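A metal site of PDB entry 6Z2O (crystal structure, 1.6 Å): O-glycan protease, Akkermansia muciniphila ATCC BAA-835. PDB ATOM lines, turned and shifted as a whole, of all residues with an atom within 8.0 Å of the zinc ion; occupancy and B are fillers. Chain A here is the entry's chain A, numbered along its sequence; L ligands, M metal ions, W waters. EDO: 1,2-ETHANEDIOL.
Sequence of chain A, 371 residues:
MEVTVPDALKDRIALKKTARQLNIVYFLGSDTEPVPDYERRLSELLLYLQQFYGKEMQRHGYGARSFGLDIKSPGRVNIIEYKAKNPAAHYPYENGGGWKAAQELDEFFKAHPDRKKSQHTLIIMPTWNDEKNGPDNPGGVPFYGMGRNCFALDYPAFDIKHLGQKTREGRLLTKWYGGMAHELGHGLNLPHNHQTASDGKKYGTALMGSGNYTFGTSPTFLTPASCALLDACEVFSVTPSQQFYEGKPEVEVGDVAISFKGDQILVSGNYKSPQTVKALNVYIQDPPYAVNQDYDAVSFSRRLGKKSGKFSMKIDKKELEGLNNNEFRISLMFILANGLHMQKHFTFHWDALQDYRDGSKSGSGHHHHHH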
ATOM      1  N   TYR A 144      -7.158  34.278   0.625  1.00  0.00           N
ATOM      2  CA  TYR A 144      -7.040  33.060   1.398  1.00  0.00           C
ATOM      3  C   TYR A 144      -6.427  33.361   2.756  1.00  0.00           C
ATOM      4  O   TYR A 144      -5.692  34.342   2.905  1.00  0.00           O
ATOM      5  CB  TYR A 144      -6.171  32.011   0.687  1.00  0.00           C
ATOM      6  CG  TYR A 144      -5.062  32.552  -0.205  1.00  0.00           C
ATOM      7  CD1 TYR A 144      -3.934  33.160   0.311  1.00  0.00           C
ATOM      8  CD2 TYR A 144      -5.147  32.420  -1.590  1.00  0.00           C
ATOM      9  CE1 TYR A 144      -2.917  33.637  -0.510  1.00  0.00           C
ATOM     10  CE2 TYR A 144      -4.148  32.871  -2.420  1.00  0.00           C
ATOM     11  CZ  TYR A 144      -3.040  33.481  -1.889  1.00  0.00           C
ATOM     12  OH  TYR A 144      -2.044  33.957  -2.717  1.00  0.00           O
ATOM     13  N   GLY A 145      -6.748  32.541   3.752  1.00  0.00           N
ATOM     14  CA  GLY A 145      -5.890  32.452   4.913  1.00  0.00           C
ATOM     15  C   GLY A 145      -4.542  31.859   4.556  1.00  0.00           C
ATOM     16  O   GLY A 145      -4.422  31.019   3.659  1.00  0.00           O
ATOM     17  N   GLY A 179     -16.669  35.782   2.013  1.00  0.00           N
ATOM     18  CA  GLY A 179     -15.343  35.219   1.807  1.00  0.00           C
ATOM     19  C   GLY A 179     -14.335  35.744   2.803  1.00  0.00           C
ATOM     20  O   GLY A 179     -13.594  34.978   3.426  1.00  0.00           O
ATOM     21  N   HIS A 182     -14.820  34.196   6.302  1.00  0.00           N
ATOM     22  CA  HIS A 182     -14.333  32.820   6.399  1.00  0.00           C
ATOM     23  C   HIS A 182     -12.820  32.769   6.321  1.00  0.00           C
ATOM     24  O   HIS A 182     -12.164  32.096   7.126  1.00  0.00           O
ATOM     25  CB  HIS A 182     -14.967  31.996   5.266  1.00  0.00           C
ATOM     26  CG  HIS A 182     -14.462  30.592   5.153  1.00  0.00           C
ATOM     27  ND1 HIS A 182     -15.170  29.510   5.626  1.00  0.00           N
ATOM     28  CD2 HIS A 182     -13.346  30.081   4.571  1.00  0.00           C
ATOM     29  CE1 HIS A 182     -14.512  28.396   5.352  1.00  0.00           C
ATOM     30  NE2 HIS A 182     -13.402  28.719   4.708  1.00  0.00           N
ATOM     31  N   GLU A 183     -12.220  33.465   5.344  1.00  0.00           N
ATOM     32  CA  GLU A 183     -10.770  33.467   5.244  1.00  0.00           C
ATOM     33  C   GLU A 183     -10.122  34.083   6.477  1.00  0.00           C
ATOM     34  O   GLU A 183      -9.064  33.618   6.918  1.00  0.00           O
ATOM     35  CB  GLU A 183     -10.324  34.188   3.970  1.00  0.00           C
ATOM     36  CG  GLU A 183     -10.862  33.568   2.666  1.00  0.00           C
ATOM     37  CD  GLU A 183     -10.561  32.068   2.559  1.00  0.00           C
ATOM     38  OE1 GLU A 183      -9.493  31.612   3.012  1.00  0.00           O
ATOM     39  OE2 GLU A 183     -11.414  31.337   2.003  1.00  0.00           O
ATOM     40  N   GLY A 185     -11.314  33.808   9.448  1.00  0.00           N
ATOM     41  CA  GLY A 185     -11.371  32.693  10.376  1.00  0.00           C
ATOM     42  C   GLY A 185     -10.153  31.793  10.275  1.00  0.00           C
ATOM     43  O   GLY A 185      -9.561  31.403  11.285  1.00  0.00           O
ATOM     44  N   HIS A 186      -9.752  31.472   9.037  1.00  0.00           N
ATOM     45  CA  HIS A 186      -8.556  30.668   8.831  1.00  0.00           C
ATOM     46  C   HIS A 186      -7.331  31.374   9.403  1.00  0.00           C
ATOM     47  O   HIS A 186      -6.497  30.754  10.083  1.00  0.00           O
ATOM     48  CB  HIS A 186      -8.359  30.376   7.344  1.00  0.00           C
ATOM     49  CG  HIS A 186      -9.264  29.313   6.775  1.00  0.00           C
ATOM     50  ND1 HIS A 186      -9.525  28.112   7.409  1.00  0.00           N
ATOM     51  CD2 HIS A 186      -9.918  29.252   5.591  1.00  0.00           C
ATOM     52  CE1 HIS A 186     -10.312  27.373   6.640  1.00  0.00           C
ATOM     53  NE2 HIS A 186     -10.564  28.042   5.522  1.00  0.00           N
ATOM     54  N   LEU A 190      -8.647  28.999  12.563  1.00  0.00           N
ATOM     55  CA  LEU A 190      -9.791  28.065  12.526  1.00  0.00           C
ATOM     56  C   LEU A 190      -9.695  27.105  11.359  1.00  0.00           C
ATOM     57  O   LEU A 190      -9.487  27.531  10.216  1.00  0.00           O
ATOM     58  CB  LEU A 190     -11.089  28.838  12.407  1.00  0.00           C
ATOM     59  CG  LEU A 190     -11.336  29.828  13.539  1.00  0.00           C
ATOM     60  CD1 LEU A 190     -12.724  30.386  13.370  1.00  0.00           C
ATOM     61  CD2 LEU A 190     -11.206  29.101  14.852  1.00  0.00           C
ATOM     62  N   PRO A 191      -9.897  25.813  11.572  1.00  0.00           N
ATOM     63  CA  PRO A 191     -10.059  24.886  10.454  1.00  0.00           C
ATOM     64  C   PRO A 191     -11.508  24.879   9.997  1.00  0.00           C
ATOM     65  O   PRO A 191     -12.393  25.517  10.570  1.00  0.00           O
ATOM     66  CB  PRO A 191      -9.663  23.546  11.074  1.00  0.00           C
ATOM     67  CG  PRO A 191     -10.175  23.646  12.473  1.00  0.00           C
ATOM     68  CD  PRO A 191      -9.916  25.119  12.872  1.00  0.00           C
ATOM     69  N   HIS A 192     -11.769  24.110   8.938  1.00  0.00           N
ATOM     70  CA  HIS A 192     -13.150  23.902   8.531  1.00  0.00           C
ATOM     71  C   HIS A 192     -13.902  23.056   9.555  1.00  0.00           C
ATOM     72  O   HIS A 192     -13.317  22.202  10.235  1.00  0.00           O
ATOM     73  CB  HIS A 192     -13.215  23.213   7.183  1.00  0.00           C
ATOM     74  CG  HIS A 192     -12.844  24.092   6.034  1.00  0.00           C
ATOM     75  ND1 HIS A 192     -12.402  23.594   4.825  1.00  0.00           N
ATOM     76  CD2 HIS A 192     -12.863  25.440   5.909  1.00  0.00           C
ATOM     77  CE1 HIS A 192     -12.158  24.607   4.009  1.00  0.00           C
ATOM     78  NE2 HIS A 192     -12.422  25.739   4.643  1.00  0.00           N
ATOM     79  N   ASN A 193     -15.213  23.276   9.643  1.00  0.00           N
ATOM     80  CA  ASN A 193     -16.070  22.359  10.427  1.00  0.00           C
ATOM     81  C   ASN A 193     -17.511  22.549   9.997  1.00  0.00           C
ATOM     82  O   ASN A 193     -17.820  23.540   9.368  1.00  0.00           O
ATOM     83  CB  ASN A 193     -15.974  22.442  11.950  1.00  0.00           C
ATOM     84  CG  ASN A 193     -16.418  23.748  12.560  1.00  0.00           C
ATOM     85  OD1 ASN A 193     -15.561  24.510  12.935  1.00  0.00           O
ATOM     86  ND2 ASN A 193     -17.708  23.997  12.678  1.00  0.00           N
ATOM     87  N   LEU A 207     -19.858  29.239   9.962  1.00  0.00           N
ATOM     88  CA  LEU A 207     -19.006  30.135   9.172  1.00  0.00           C
ATOM     89  C   LEU A 207     -17.866  29.375   8.506  1.00  0.00           C
ATOM     90  O   LEU A 207     -17.529  29.646   7.337  1.00  0.00           O
ATOM     91  CB  LEU A 207     -18.430  31.250  10.041  1.00  0.00           C
ATOM     92  CG  LEU A 207     -17.480  32.178   9.276  1.00  0.00           C
ATOM     93  CD1 LEU A 207     -18.207  32.945   8.166  1.00  0.00           C
ATOM     94  CD2 LEU A 207     -16.782  33.162  10.221  1.00  0.00           C
ATOM     95  N   MET A 208     -17.247  28.453   9.226  1.00  0.00           N
ATOM     96  CA  MET A 208     -16.080  27.755   8.715  1.00  0.00           C
ATOM     97  C   MET A 208     -16.438  26.466   7.976  1.00  0.00           C
ATOM     98  O   MET A 208     -15.574  25.622   7.764  1.00  0.00           O
ATOM     99  CB  MET A 208     -15.083  27.470   9.849  1.00  0.00           C
ATOM    100  CG  MET A 208     -14.529  28.745  10.531  1.00  0.00           C
ATOM    101  SD  MET A 208     -13.893  29.976   9.376  1.00  0.00           S
ATOM    102  CE  MET A 208     -12.618  28.990   8.577  1.00  0.00           C
ATOM    103  N   GLY A 209     -17.692  26.332   7.530  1.00  0.00           N
ATOM    104  CA  GLY A 209     -18.051  25.207   6.680  1.00  0.00           C
ATOM    105  C   GLY A 209     -17.402  25.315   5.307  1.00  0.00           C
ATOM    106  O   GLY A 209     -17.055  26.398   4.844  1.00  0.00           O
ATOM    107  N   SER A 210     -17.227  24.159   4.660  1.00  0.00           N
ATOM    108  CA  SER A 210     -16.490  24.123   3.390  1.00  0.00           C
ATOM    109  C   SER A 210     -17.352  24.495   2.192  1.00  0.00           C
ATOM    110  O   SER A 210     -16.805  24.618   1.083  1.00  0.00           O
ATOM    111  CB  SER A 210     -15.878  22.735   3.185  1.00  0.00           C
ATOM    112  N   GLY A 211     -18.654  24.705   2.367  1.00  0.00           N
ATOM    113  CA  GLY A 211     -19.532  25.060   1.273  1.00  0.00           C
ATOM    114  C   GLY A 211     -19.385  26.518   0.870  1.00  0.00           C
ATOM    115  O   GLY A 211     -18.411  27.194   1.186  1.00  0.00           O
ATOM    116  N   TYR A 213     -19.949  30.526   0.681  1.00  0.00           N
ATOM    117  CA  TYR A 213     -20.007  31.535   1.728  1.00  0.00           C
ATOM    118  C   TYR A 213     -21.453  31.943   1.986  1.00  0.00           C
ATOM    119  O   TYR A 213     -22.225  32.179   1.049  1.00  0.00           O
ATOM    120  CB  TYR A 213     -19.165  32.753   1.319  1.00  0.00           C
ATOM    121  CG  TYR A 213     -17.696  32.473   1.008  1.00  0.00           C
ATOM    122  CD1 TYR A 213     -16.884  31.819   1.922  1.00  0.00           C
ATOM    123  CD2 TYR A 213     -17.123  32.896  -0.200  1.00  0.00           C
ATOM    124  CE1 TYR A 213     -15.524  31.581   1.644  1.00  0.00           C
ATOM    125  CE2 TYR A 213     -15.763  32.667  -0.494  1.00  0.00           C
ATOM    126  CZ  TYR A 213     -14.973  32.002   0.428  1.00  0.00           C
ATOM    127  OH  TYR A 213     -13.636  31.778   0.158  1.00  0.00           O
HETATM  128  C1  EDO L   1     -13.630  28.031   1.138  1.00  0.00           C
HETATM  129  O1  EDO L   1     -13.101  27.300   2.238  1.00  0.00           O
HETATM  130  C2  EDO L   1     -15.004  27.469   0.772  1.00  0.00           C
HETATM  131  O2  EDO L   1     -15.517  28.198  -0.356  1.00  0.00           O
HETATM  132 ZN    ZN M   1     -11.878  27.517   3.907  1.00  0.00          ZN
HETATM  133  O   HOH W   1     -11.061  28.977   2.718  1.00  0.00           O
HETATM  134  O   HOH W   2     -10.170  26.404   2.890  1.00  0.00           O
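Three residues have an atom within 4 Å of the zinc ion: His 182, His 186 and His 192.
Along chain A the residues within 4 Å of the zinc ion span positions 182 to 192.
The zinc ion is bound by NE2 of His 192 (2.0 Å), water W1 (2.1 Å), O1 of the ligand (2.1 Å), NE2 of His 182 (2.1 Å), NE2 of His 186 (2.1 Å) and water W2 (2.3 Å).
The zinc ion has six donor atoms within binding distance.
ND1 of His 182 lies within hydrogen-bond range of O of Leu 207 (2.9 Å).
A ring nitrogen (ND1) of His 186 lies within hydrogen-bond range of the backbone carbonyl oxygen (O) of Leu 190, 2.9 Å away.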
